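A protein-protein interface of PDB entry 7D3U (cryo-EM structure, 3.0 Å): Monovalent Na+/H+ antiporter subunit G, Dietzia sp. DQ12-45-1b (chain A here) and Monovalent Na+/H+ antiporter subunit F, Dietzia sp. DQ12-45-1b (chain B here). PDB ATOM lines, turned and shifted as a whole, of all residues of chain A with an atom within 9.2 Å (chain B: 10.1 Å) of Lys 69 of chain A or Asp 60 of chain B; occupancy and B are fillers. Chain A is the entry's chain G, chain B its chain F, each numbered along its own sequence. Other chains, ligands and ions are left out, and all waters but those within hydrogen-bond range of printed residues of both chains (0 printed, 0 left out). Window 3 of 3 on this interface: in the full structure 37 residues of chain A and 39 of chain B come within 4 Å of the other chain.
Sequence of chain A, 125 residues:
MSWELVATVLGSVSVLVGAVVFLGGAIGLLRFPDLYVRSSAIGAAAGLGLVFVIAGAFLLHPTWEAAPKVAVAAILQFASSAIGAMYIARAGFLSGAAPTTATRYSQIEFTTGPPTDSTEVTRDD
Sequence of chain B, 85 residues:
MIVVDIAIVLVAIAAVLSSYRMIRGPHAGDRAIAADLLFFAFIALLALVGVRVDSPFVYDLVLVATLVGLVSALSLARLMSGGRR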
ATOM      1  N   ILE A  54      32.194  27.156  -7.944  1.00  0.00           N
ATOM      2  CA  ILE A  54      30.743  27.304  -7.877  1.00  0.00           C
ATOM      3  C   ILE A  54      30.339  28.009  -6.589  1.00  0.00           C
ATOM      4  O   ILE A  54      29.551  28.963  -6.603  1.00  0.00           O
ATOM      5  CB  ILE A  54      30.056  25.933  -8.007  1.00  0.00           C
ATOM      6  CG1 ILE A  54      30.166  25.419  -9.439  1.00  0.00           C
ATOM      7  CG2 ILE A  54      28.600  26.023  -7.593  1.00  0.00           C
ATOM      8  CD1 ILE A  54      29.731  26.411 -10.473  1.00  0.00           C
ATOM      9  N   PHE A  58      28.701  31.723  -6.149  1.00  0.00           N
ATOM     10  CA  PHE A  58      27.444  31.912  -5.434  1.00  0.00           C
ATOM     11  C   PHE A  58      27.593  32.939  -4.323  1.00  0.00           C
ATOM     12  O   PHE A  58      26.684  33.739  -4.082  1.00  0.00           O
ATOM     13  CB  PHE A  58      26.953  30.581  -4.872  1.00  0.00           C
ATOM     14  CG  PHE A  58      25.770  30.712  -3.963  1.00  0.00           C
ATOM     15  CD1 PHE A  58      24.544  31.111  -4.459  1.00  0.00           C
ATOM     16  CD2 PHE A  58      25.882  30.437  -2.613  1.00  0.00           C
ATOM     17  CE1 PHE A  58      23.452  31.232  -3.629  1.00  0.00           C
ATOM     18  CE2 PHE A  58      24.795  30.557  -1.777  1.00  0.00           C
ATOM     19  CZ  PHE A  58      23.578  30.955  -2.285  1.00  0.00           C
ATOM     20  N   THR A  63      22.037  35.088  -4.358  1.00  0.00           N
ATOM     21  CA  THR A  63      20.591  35.098  -4.504  1.00  0.00           C
ATOM     22  C   THR A  63      19.974  33.993  -3.652  1.00  0.00           C
ATOM     23  O   THR A  63      20.640  33.041  -3.240  1.00  0.00           O
ATOM     24  CB  THR A  63      20.191  34.921  -5.969  1.00  0.00           C
ATOM     25  OG1 THR A  63      20.927  33.833  -6.540  1.00  0.00           O
ATOM     26  CG2 THR A  63      20.478  36.189  -6.757  1.00  0.00           C
ATOM     27  N   TRP A  64      18.677  34.130  -3.388  1.00  0.00           N
ATOM     28  CA  TRP A  64      17.981  33.173  -2.541  1.00  0.00           C
ATOM     29  C   TRP A  64      17.338  32.040  -3.325  1.00  0.00           C
ATOM     30  O   TRP A  64      17.073  30.979  -2.749  1.00  0.00           O
ATOM     31  CB  TRP A  64      16.913  33.884  -1.707  1.00  0.00           C
ATOM     32  CG  TRP A  64      16.799  33.354  -0.314  1.00  0.00           C
ATOM     33  CD1 TRP A  64      15.764  32.636   0.208  1.00  0.00           C
ATOM     34  CD2 TRP A  64      17.759  33.498   0.739  1.00  0.00           C
ATOM     35  NE1 TRP A  64      16.019  32.324   1.521  1.00  0.00           N
ATOM     36  CE2 TRP A  64      17.237  32.843   1.871  1.00  0.00           C
ATOM     37  CE3 TRP A  64      19.007  34.119   0.835  1.00  0.00           C
ATOM     38  CZ2 TRP A  64      17.921  32.788   3.082  1.00  0.00           C
ATOM     39  CZ3 TRP A  64      19.684  34.064   2.037  1.00  0.00           C
ATOM     40  CH2 TRP A  64      19.139  33.404   3.145  1.00  0.00           C
ATOM     41  N   GLU A  65      17.079  32.238  -4.614  1.00  0.00           N
ATOM     42  CA  GLU A  65      16.458  31.224  -5.453  1.00  0.00           C
ATOM     43  C   GLU A  65      17.466  30.264  -6.070  1.00  0.00           C
ATOM     44  O   GLU A  65      17.059  29.301  -6.726  1.00  0.00           O
ATOM     45  CB  GLU A  65      15.642  31.888  -6.565  1.00  0.00           C
ATOM     46  CG  GLU A  65      16.412  32.936  -7.352  1.00  0.00           C
ATOM     47  CD  GLU A  65      15.594  33.548  -8.473  1.00  0.00           C
ATOM     48  OE1 GLU A  65      15.035  32.785  -9.289  1.00  0.00           O
ATOM     49  OE2 GLU A  65      15.510  34.791  -8.539  1.00  0.00           O
ATOM     50  N   ALA A  66      18.762  30.501  -5.880  1.00  0.00           N
ATOM     51  CA  ALA A  66      19.802  29.662  -6.456  1.00  0.00           C
ATOM     52  C   ALA A  66      20.526  28.813  -5.424  1.00  0.00           C
ATOM     53  O   ALA A  66      21.480  28.113  -5.778  1.00  0.00           O
ATOM     54  CB  ALA A  66      20.816  30.523  -7.216  1.00  0.00           C
ATOM     55  N   ALA A  67      20.104  28.853  -4.157  1.00  0.00           N
ATOM     56  CA  ALA A  67      20.785  28.052  -3.141  1.00  0.00           C
ATOM     57  C   ALA A  67      20.546  26.558  -3.326  1.00  0.00           C
ATOM     58  O   ALA A  67      21.519  25.788  -3.254  1.00  0.00           O
ATOM     59  CB  ALA A  67      20.381  28.527  -1.743  1.00  0.00           C
ATOM     60  N   PRO A  68      19.317  26.073  -3.555  1.00  0.00           N
ATOM     61  CA  PRO A  68      19.167  24.632  -3.822  1.00  0.00           C
ATOM     62  C   PRO A  68      19.867  24.188  -5.093  1.00  0.00           C
ATOM     63  O   PRO A  68      20.459  23.101  -5.127  1.00  0.00           O
ATOM     64  CB  PRO A  68      17.646  24.451  -3.918  1.00  0.00           C
ATOM     65  CG  PRO A  68      17.081  25.594  -3.167  1.00  0.00           C
ATOM     66  CD  PRO A  68      18.005  26.733  -3.446  1.00  0.00           C
ATOM     67  N   LYS A  69      19.823  25.007  -6.143  1.00  0.00           N
ATOM     68  CA  LYS A  69      20.479  24.682  -7.402  1.00  0.00           C
ATOM     69  C   LYS A  69      21.997  24.737  -7.311  1.00  0.00           C
ATOM     70  O   LYS A  69      22.668  24.426  -8.300  1.00  0.00           O
ATOM     71  CB  LYS A  69      19.983  25.623  -8.499  1.00  0.00           C
ATOM     72  CG  LYS A  69      18.536  25.382  -8.885  1.00  0.00           C
ATOM     73  CD  LYS A  69      18.103  26.293 -10.015  1.00  0.00           C
ATOM     74  CE  LYS A  69      17.665  27.649  -9.492  1.00  0.00           C
ATOM     75  NZ  LYS A  69      16.379  27.568  -8.749  1.00  0.00           N
ATOM     76  N   VAL A  70      22.548  25.132  -6.166  1.00  0.00           N
ATOM     77  CA  VAL A  70      23.973  25.031  -5.902  1.00  0.00           C
ATOM     78  C   VAL A  70      24.275  23.917  -4.907  1.00  0.00           C
ATOM     79  O   VAL A  70      25.270  23.203  -5.052  1.00  0.00           O
ATOM     80  CB  VAL A  70      24.534  26.383  -5.410  1.00  0.00           C
ATOM     81  CG1 VAL A  70      25.831  26.193  -4.645  1.00  0.00           C
ATOM     82  CG2 VAL A  70      24.746  27.316  -6.584  1.00  0.00           C
ATOM     83  N   ALA A  71      23.412  23.738  -3.903  1.00  0.00           N
ATOM     84  CA  ALA A  71      23.579  22.628  -2.973  1.00  0.00           C
ATOM     85  C   ALA A  71      23.477  21.285  -3.681  1.00  0.00           C
ATOM     86  O   ALA A  71      24.171  20.334  -3.310  1.00  0.00           O
ATOM     87  CB  ALA A  71      22.543  22.719  -1.854  1.00  0.00           C
ATOM     88  N   VAL A  72      22.618  21.186  -4.695  1.00  0.00           N
ATOM     89  CA  VAL A  72      22.553  19.965  -5.491  1.00  0.00           C
ATOM     90  C   VAL A  72      23.722  19.901  -6.464  1.00  0.00           C
ATOM     91  O   VAL A  72      24.301  18.829  -6.694  1.00  0.00           O
ATOM     92  CB  VAL A  72      21.199  19.886  -6.220  1.00  0.00           C
ATOM     93  CG1 VAL A  72      21.232  18.831  -7.311  1.00  0.00           C
ATOM     94  CG2 VAL A  72      20.084  19.599  -5.232  1.00  0.00           C
ATOM     95  N   ALA A  73      24.089  21.049  -7.039  1.00  0.00           N
ATOM     96  CA  ALA A  73      25.138  21.078  -8.050  1.00  0.00           C
ATOM     97  C   ALA A  73      26.480  20.653  -7.473  1.00  0.00           C
ATOM     98  O   ALA A  73      27.269  19.997  -8.156  1.00  0.00           O
ATOM     99  CB  ALA A  73      25.239  22.472  -8.663  1.00  0.00           C
ATOM    100  N   ALA A  74      26.764  21.017  -6.223  1.00  0.00           N
ATOM    101  CA  ALA A  74      28.048  20.657  -5.626  1.00  0.00           C
ATOM    102  C   ALA A  74      28.181  19.146  -5.478  1.00  0.00           C
ATOM    103  O   ALA A  74      29.202  18.554  -5.856  1.00  0.00           O
ATOM    104  CB  ALA A  74      28.209  21.352  -4.274  1.00  0.00           C
ATOM    105  N   ILE A  75      27.153  18.504  -4.920  1.00  0.00           N
ATOM    106  CA  ILE A  75      27.180  17.054  -4.751  1.00  0.00           C
ATOM    107  C   ILE A  75      27.246  16.363  -6.105  1.00  0.00           C
ATOM    108  O   ILE A  75      27.977  15.377  -6.284  1.00  0.00           O
ATOM    109  CB  ILE A  75      25.955  16.593  -3.942  1.00  0.00           C
ATOM    110  CG1 ILE A  75      25.918  17.301  -2.589  1.00  0.00           C
ATOM    111  CG2 ILE A  75      25.976  15.087  -3.758  1.00  0.00           C
ATOM    112  CD1 ILE A  75      24.698  16.969  -1.764  1.00  0.00           C
ATOM    113  N   LEU A  76      26.487  16.867  -7.082  1.00  0.00           N
ATOM    114  CA  LEU A  76      26.519  16.262  -8.408  1.00  0.00           C
ATOM    115  C   LEU A  76      27.888  16.418  -9.053  1.00  0.00           C
ATOM    116  O   LEU A  76      28.375  15.494  -9.708  1.00  0.00           O
ATOM    117  CB  LEU A  76      25.430  16.869  -9.289  1.00  0.00           C
ATOM    118  CG  LEU A  76      24.007  16.436  -8.941  1.00  0.00           C
ATOM    119  CD1 LEU A  76      23.043  16.860 -10.029  1.00  0.00           C
ATOM    120  CD2 LEU A  76      23.943  14.934  -8.721  1.00  0.00           C
ATOM    121  N   GLN A  77      28.534  17.570  -8.860  1.00  0.00           N
ATOM    122  CA  GLN A  77      29.871  17.773  -9.402  1.00  0.00           C
ATOM    123  C   GLN A  77      30.864  16.808  -8.778  1.00  0.00           C
ATOM    124  O   GLN A  77      31.691  16.220  -9.480  1.00  0.00           O
ATOM    125  CB  GLN A  77      30.323  19.212  -9.171  1.00  0.00           C
ATOM    126  CG  GLN A  77      29.533  20.235  -9.951  1.00  0.00           C
ATOM    127  CD  GLN A  77      29.961  21.652  -9.641  1.00  0.00           C
ATOM    128  OE1 GLN A  77      30.491  21.933  -8.572  1.00  0.00           O
ATOM    129  NE2 GLN A  77      29.732  22.556 -10.578  1.00  0.00           N
ATOM    130  N   ILE B  43      32.372  24.533 -17.058  1.00  0.00           N
ATOM    131  CA  ILE B  43      31.368  24.855 -16.046  1.00  0.00           C
ATOM    132  C   ILE B  43      31.879  25.958 -15.125  1.00  0.00           C
ATOM    133  O   ILE B  43      31.144  26.894 -14.773  1.00  0.00           O
ATOM    134  CB  ILE B  43      30.975  23.595 -15.255  1.00  0.00           C
ATOM    135  CG1 ILE B  43      30.496  22.501 -16.203  1.00  0.00           C
ATOM    136  CG2 ILE B  43      29.893  23.919 -14.247  1.00  0.00           C
ATOM    137  CD1 ILE B  43      30.127  21.220 -15.502  1.00  0.00           C
ATOM    138  N   LEU B  46      31.579  29.149 -16.968  1.00  0.00           N
ATOM    139  CA  LEU B  46      30.187  29.586 -16.960  1.00  0.00           C
ATOM    140  C   LEU B  46      29.866  30.330 -15.674  1.00  0.00           C
ATOM    141  O   LEU B  46      29.302  31.430 -15.701  1.00  0.00           O
ATOM    142  CB  LEU B  46      29.256  28.387 -17.129  1.00  0.00           C
ATOM    143  CG  LEU B  46      28.979  27.900 -18.549  1.00  0.00           C
ATOM    144  CD1 LEU B  46      27.964  26.771 -18.533  1.00  0.00           C
ATOM    145  CD2 LEU B  46      28.484  29.044 -19.406  1.00  0.00           C
ATOM    146  N   ALA B  47      30.236  29.746 -14.534  1.00  0.00           N
ATOM    147  CA  ALA B  47      29.964  30.390 -13.251  1.00  0.00           C
ATOM    148  C   ALA B  47      30.662  31.742 -13.148  1.00  0.00           C
ATOM    149  O   ALA B  47      30.043  32.756 -12.797  1.00  0.00           O
ATOM    150  CB  ALA B  47      30.397  29.477 -12.107  1.00  0.00           C
ATOM    151  N   SER B  55      24.362  38.056 -13.692  1.00  0.00           N
ATOM    152  CA  SER B  55      23.192  37.378 -14.208  1.00  0.00           C
ATOM    153  C   SER B  55      22.613  36.498 -13.107  1.00  0.00           C
ATOM    154  O   SER B  55      23.369  35.783 -12.427  1.00  0.00           O
ATOM    155  CB  SER B  55      23.539  36.536 -15.437  1.00  0.00           C
ATOM    156  OG  SER B  55      22.414  36.373 -16.281  1.00  0.00           O
ATOM    157  N   PRO B  56      21.294  36.531 -12.894  1.00  0.00           N
ATOM    158  CA  PRO B  56      20.696  35.632 -11.900  1.00  0.00           C
ATOM    159  C   PRO B  56      20.511  34.213 -12.401  1.00  0.00           C
ATOM    160  O   PRO B  56      20.480  33.285 -11.581  1.00  0.00           O
ATOM    161  CB  PRO B  56      19.337  36.286 -11.601  1.00  0.00           C
ATOM    162  CG  PRO B  56      19.379  37.642 -12.268  1.00  0.00           C
ATOM    163  CD  PRO B  56      20.319  37.498 -13.413  1.00  0.00           C
ATOM    164  N   PHE B  57      20.382  34.017 -13.707  1.00  0.00           N
ATOM    165  CA  PHE B  57      20.082  32.712 -14.295  1.00  0.00           C
ATOM    166  C   PHE B  57      21.350  31.981 -14.712  1.00  0.00           C
ATOM    167  O   PHE B  57      21.491  31.548 -15.854  1.00  0.00           O
ATOM    168  CB  PHE B  57      19.139  32.887 -15.477  1.00  0.00           C
ATOM    169  CG  PHE B  57      18.156  34.003 -15.293  1.00  0.00           C
ATOM    170  CD1 PHE B  57      16.969  33.791 -14.616  1.00  0.00           C
ATOM    171  CD2 PHE B  57      18.428  35.269 -15.780  1.00  0.00           C
ATOM    172  CE1 PHE B  57      16.066  34.818 -14.438  1.00  0.00           C
ATOM    173  CE2 PHE B  57      17.532  36.298 -15.604  1.00  0.00           C
ATOM    174  CZ  PHE B  57      16.348  36.074 -14.932  1.00  0.00           C
ATOM    175  N   VAL B  58      22.294  31.837 -13.789  1.00  0.00           N
ATOM    176  CA  VAL B  58      23.529  31.116 -14.074  1.00  0.00           C
ATOM    177  C   VAL B  58      23.420  29.654 -13.675  1.00  0.00           C
ATOM    178  O   VAL B  58      23.703  28.755 -14.470  1.00  0.00           O
ATOM    179  CB  VAL B  58      24.715  31.797 -13.365  1.00  0.00           C
ATOM    180  CG1 VAL B  58      26.007  31.095 -13.718  1.00  0.00           C
ATOM    181  CG2 VAL B  58      24.785  33.255 -13.746  1.00  0.00           C
ATOM    182  N   TYR B  59      22.987  29.400 -12.442  1.00  0.00           N
ATOM    183  CA  TYR B  59      23.145  28.074 -11.862  1.00  0.00           C
ATOM    184  C   TYR B  59      22.199  27.051 -12.464  1.00  0.00           C
ATOM    185  O   TYR B  59      22.488  25.851 -12.386  1.00  0.00           O
ATOM    186  CB  TYR B  59      22.993  28.170 -10.350  1.00  0.00           C
ATOM    187  CG  TYR B  59      24.120  28.986  -9.791  1.00  0.00           C
ATOM    188  CD1 TYR B  59      25.424  28.524  -9.869  1.00  0.00           C
ATOM    189  CD2 TYR B  59      23.899  30.244  -9.257  1.00  0.00           C
ATOM    190  CE1 TYR B  59      26.467  29.268  -9.394  1.00  0.00           C
ATOM    191  CE2 TYR B  59      24.941  30.999  -8.777  1.00  0.00           C
ATOM    192  CZ  TYR B  59      26.222  30.503  -8.850  1.00  0.00           C
ATOM    193  OH  TYR B  59      27.274  31.242  -8.382  1.00  0.00           O
ATOM    194  N   ASP B  60      21.092  27.489 -13.065  1.00  0.00           N
ATOM    195  CA  ASP B  60      20.339  26.608 -13.948  1.00  0.00           C
ATOM    196  C   ASP B  60      21.290  25.892 -14.896  1.00  0.00           C
ATOM    197  O   ASP B  60      21.386  24.660 -14.896  1.00  0.00           O
ATOM    198  CB  ASP B  60      19.298  27.411 -14.730  1.00  0.00           C
ATOM    199  CG  ASP B  60      18.471  28.311 -13.839  1.00  0.00           C
ATOM    200  OD1 ASP B  60      18.396  28.038 -12.625  1.00  0.00           O
ATOM    201  OD2 ASP B  60      17.896  29.294 -14.350  1.00  0.00           O
ATOM    202  N   LEU B  61      22.046  26.670 -15.674  1.00  0.00           N
ATOM    203  CA  LEU B  61      23.083  26.105 -16.529  1.00  0.00           C
ATOM    204  C   LEU B  61      24.045  25.243 -15.721  1.00  0.00           C
ATOM    205  O   LEU B  61      24.391  24.128 -16.126  1.00  0.00           O
ATOM    206  CB  LEU B  61      23.839  27.228 -17.237  1.00  0.00           C
ATOM    207  CG  LEU B  61      22.984  28.229 -18.006  1.00  0.00           C
ATOM    208  CD1 LEU B  61      23.825  29.407 -18.440  1.00  0.00           C
ATOM    209  CD2 LEU B  61      22.348  27.560 -19.204  1.00  0.00           C
ATOM    210  N   VAL B  62      24.469  25.740 -14.557  1.00  0.00           N
ATOM    211  CA  VAL B  62      25.394  24.972 -13.733  1.00  0.00           C
ATOM    212  C   VAL B  62      24.729  23.696 -13.242  1.00  0.00           C
ATOM    213  O   VAL B  62      25.381  22.650 -13.135  1.00  0.00           O
ATOM    214  CB  VAL B  62      25.913  25.836 -12.571  1.00  0.00           C
ATOM    215  CG1 VAL B  62      26.574  24.974 -11.513  1.00  0.00           C
ATOM    216  CG2 VAL B  62      26.882  26.882 -13.089  1.00  0.00           C
ATOM    217  N   LEU B  63      23.426  23.741 -12.966  1.00  0.00           N
ATOM    218  CA  LEU B  63      22.724  22.521 -12.593  1.00  0.00           C
ATOM    219  C   LEU B  63      22.574  21.576 -13.776  1.00  0.00           C
ATOM    220  O   LEU B  63      22.426  20.366 -13.577  1.00  0.00           O
ATOM    221  CB  LEU B  63      21.355  22.859 -12.006  1.00  0.00           C
ATOM    222  CG  LEU B  63      20.532  21.697 -11.457  1.00  0.00           C
ATOM    223  CD1 LEU B  63      21.369  20.871 -10.501  1.00  0.00           C
ATOM    224  CD2 LEU B  63      19.284  22.213 -10.768  1.00  0.00           C
ATOM    225  N   VAL B  64      22.624  22.099 -14.998  1.00  0.00           N
ATOM    226  CA  VAL B  64      22.445  21.276 -16.188  1.00  0.00           C
ATOM    227  C   VAL B  64      23.782  20.829 -16.763  1.00  0.00           C
ATOM    228  O   VAL B  64      23.925  19.680 -17.185  1.00  0.00           O
ATOM    229  CB  VAL B  64      21.610  22.047 -17.227  1.00  0.00           C
ATOM    230  CG1 VAL B  64      21.727  21.397 -18.591  1.00  0.00           C
ATOM    231  CG2 VAL B  64      20.165  22.113 -16.782  1.00  0.00           C
ATOM    232  N   ALA B  65      24.775  21.722 -16.783  1.00  0.00           N
ATOM    233  CA  ALA B  65      26.075  21.373 -17.346  1.00  0.00           C
ATOM    234  C   ALA B  65      26.703  20.189 -16.624  1.00  0.00           C
ATOM    235  O   ALA B  65      27.416  19.393 -17.245  1.00  0.00           O
ATOM    236  CB  ALA B  65      27.010  22.579 -17.302  1.00  0.00           C
ATOM    237  N   THR B  66      26.448  20.050 -15.323  1.00  0.00           N
ATOM    238  CA  THR B  66      26.953  18.891 -14.595  1.00  0.00           C
ATOM    239  C   THR B  66      26.271  17.613 -15.061  1.00  0.00           C
ATOM    240  O   THR B  66      26.912  16.561 -15.155  1.00  0.00           O
ATOM    241  CB  THR B  66      26.760  19.089 -13.096  1.00  0.00           C
ATOM    242  OG1 THR B  66      25.365  19.240 -12.814  1.00  0.00           O
ATOM    243  CG2 THR B  66      27.489  20.329 -12.646  1.00  0.00           C
ATOM    244  N   LEU B  67      24.975  17.685 -15.359  1.00  0.00           N
ATOM    245  CA  LEU B  67      24.288  16.574 -16.004  1.00  0.00           C
ATOM    246  C   LEU B  67      24.664  16.434 -17.468  1.00  0.00           C
ATOM    247  O   LEU B  67      24.170  15.519 -18.133  1.00  0.00           O
ATOM    248  CB  LEU B  67      22.775  16.744 -15.882  1.00  0.00           C
ATOM    249  CG  LEU B  67      22.233  16.965 -14.472  1.00  0.00           C
ATOM    250  CD1 LEU B  67      20.721  16.869 -14.473  1.00  0.00           C
ATOM    251  CD2 LEU B  67      22.833  15.956 -13.515  1.00  0.00           C
ATOM    252  N   VAL B  68      25.512  17.321 -17.981  1.00  0.00           N
ATOM    253  CA  VAL B  68      25.973  17.267 -19.355  1.00  0.00           C
ATOM    254  C   VAL B  68      27.455  16.920 -19.432  1.00  0.00           C
ATOM    255  O   VAL B  68      27.858  16.090 -20.249  1.00  0.00           O
ATOM    256  CB  VAL B  68      25.677  18.599 -20.077  1.00  0.00           C
ATOM    257  CG1 VAL B  68      26.563  18.760 -21.290  1.00  0.00           C
ATOM    258  CG2 VAL B  68      24.214  18.668 -20.471  1.00  0.00           C
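The backbone carbonyl oxygen (O) of Val 62 of chain B lies close to the side-chain hydroxyl (OG1) of Thr 66 of chain B (3.4 Å). The side-chain amino group (NZ) of Lys 69 of chain A lies within hydrogen-bond range of the backbone carbonyl oxygen (O) of Glu 65 of chain A, at 2.7 Å. OG1 of Thr 66 of chain B is in hydrogen-bond range of O of Leu 63 of chain B, at 3.2 Å.
Of the 17 printed residues of chain B, 8 touch a printed residue of chain A. Hydrophobic or aromatic side chains of chain B that line the printed part of chain A: Ile 43, Ala 47, Tyr 59, Val 62, Leu 63 and Leu 67. Along chain B the printed residues that touch a printed residue of chain A span positions 43 to 67.
Among the printed residues, pairs that only touch across the chains: Ile 54 of chain A with Ala 47 of chain B, Ile 54 of chain A with Tyr 59 of chain B, Ile 54 of chain A with Val 62 of chain B, Ala 66 of chain A with Tyr 59 of chain B, Lys 69 of chain A with Asp 60 of chain B, Lys 69 of chain A with Leu 63 of chain B, Val 70 of chain A with Tyr 59 of chain B, Val 72 of chain A with Leu 63 of chain B, Leu 76 of chain A with Leu 67 of chain B, Gln 77 of chain A with Ile 43 of chain B and Gln 77 of chain A with Thr 66 of chain B.
The side-chain hydroxyl (OH) of Tyr 59 of chain B lies within hydrogen-bond range of the backbone NH (N) of Phe 58 of chain A.
Printed residues of chain B within 4 Å of Ile 54 of chain A: Ala 47, Tyr 59 and Val 62. Thr 63 of chain A touches none of the printed residues of chain B. Of the printed residues of chain B, Ala 66 of chain A touches Tyr 59 (3.7 Å). Ala 67 of chain A touches none of the printed residues of chain B. Lys 69 of chain A touches just these residues of chain B: Asp 60 and Leu 63. Ala 74 of chain A touches none of the printed residues of chain B. Printed residues of chain A within 4 Å of Val 62 of chain B: Ile 54. Leu 63 of chain B touches just these residues of chain A: Lys 69 (3.8 Å) and Val 72 (3.8 Å). Printed residues of chain A within 4 Å of Leu 67 of chain B: Leu 76 (3.6 Å). The nearest residue of chain B that does not touch Lys 69 of chain A is Tyr 59 of chain B (4.3 Å). The nearest printed residue of chain B that does not touch Phe 58 of chain A is Ala 47 of chain B (6.6 Å).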
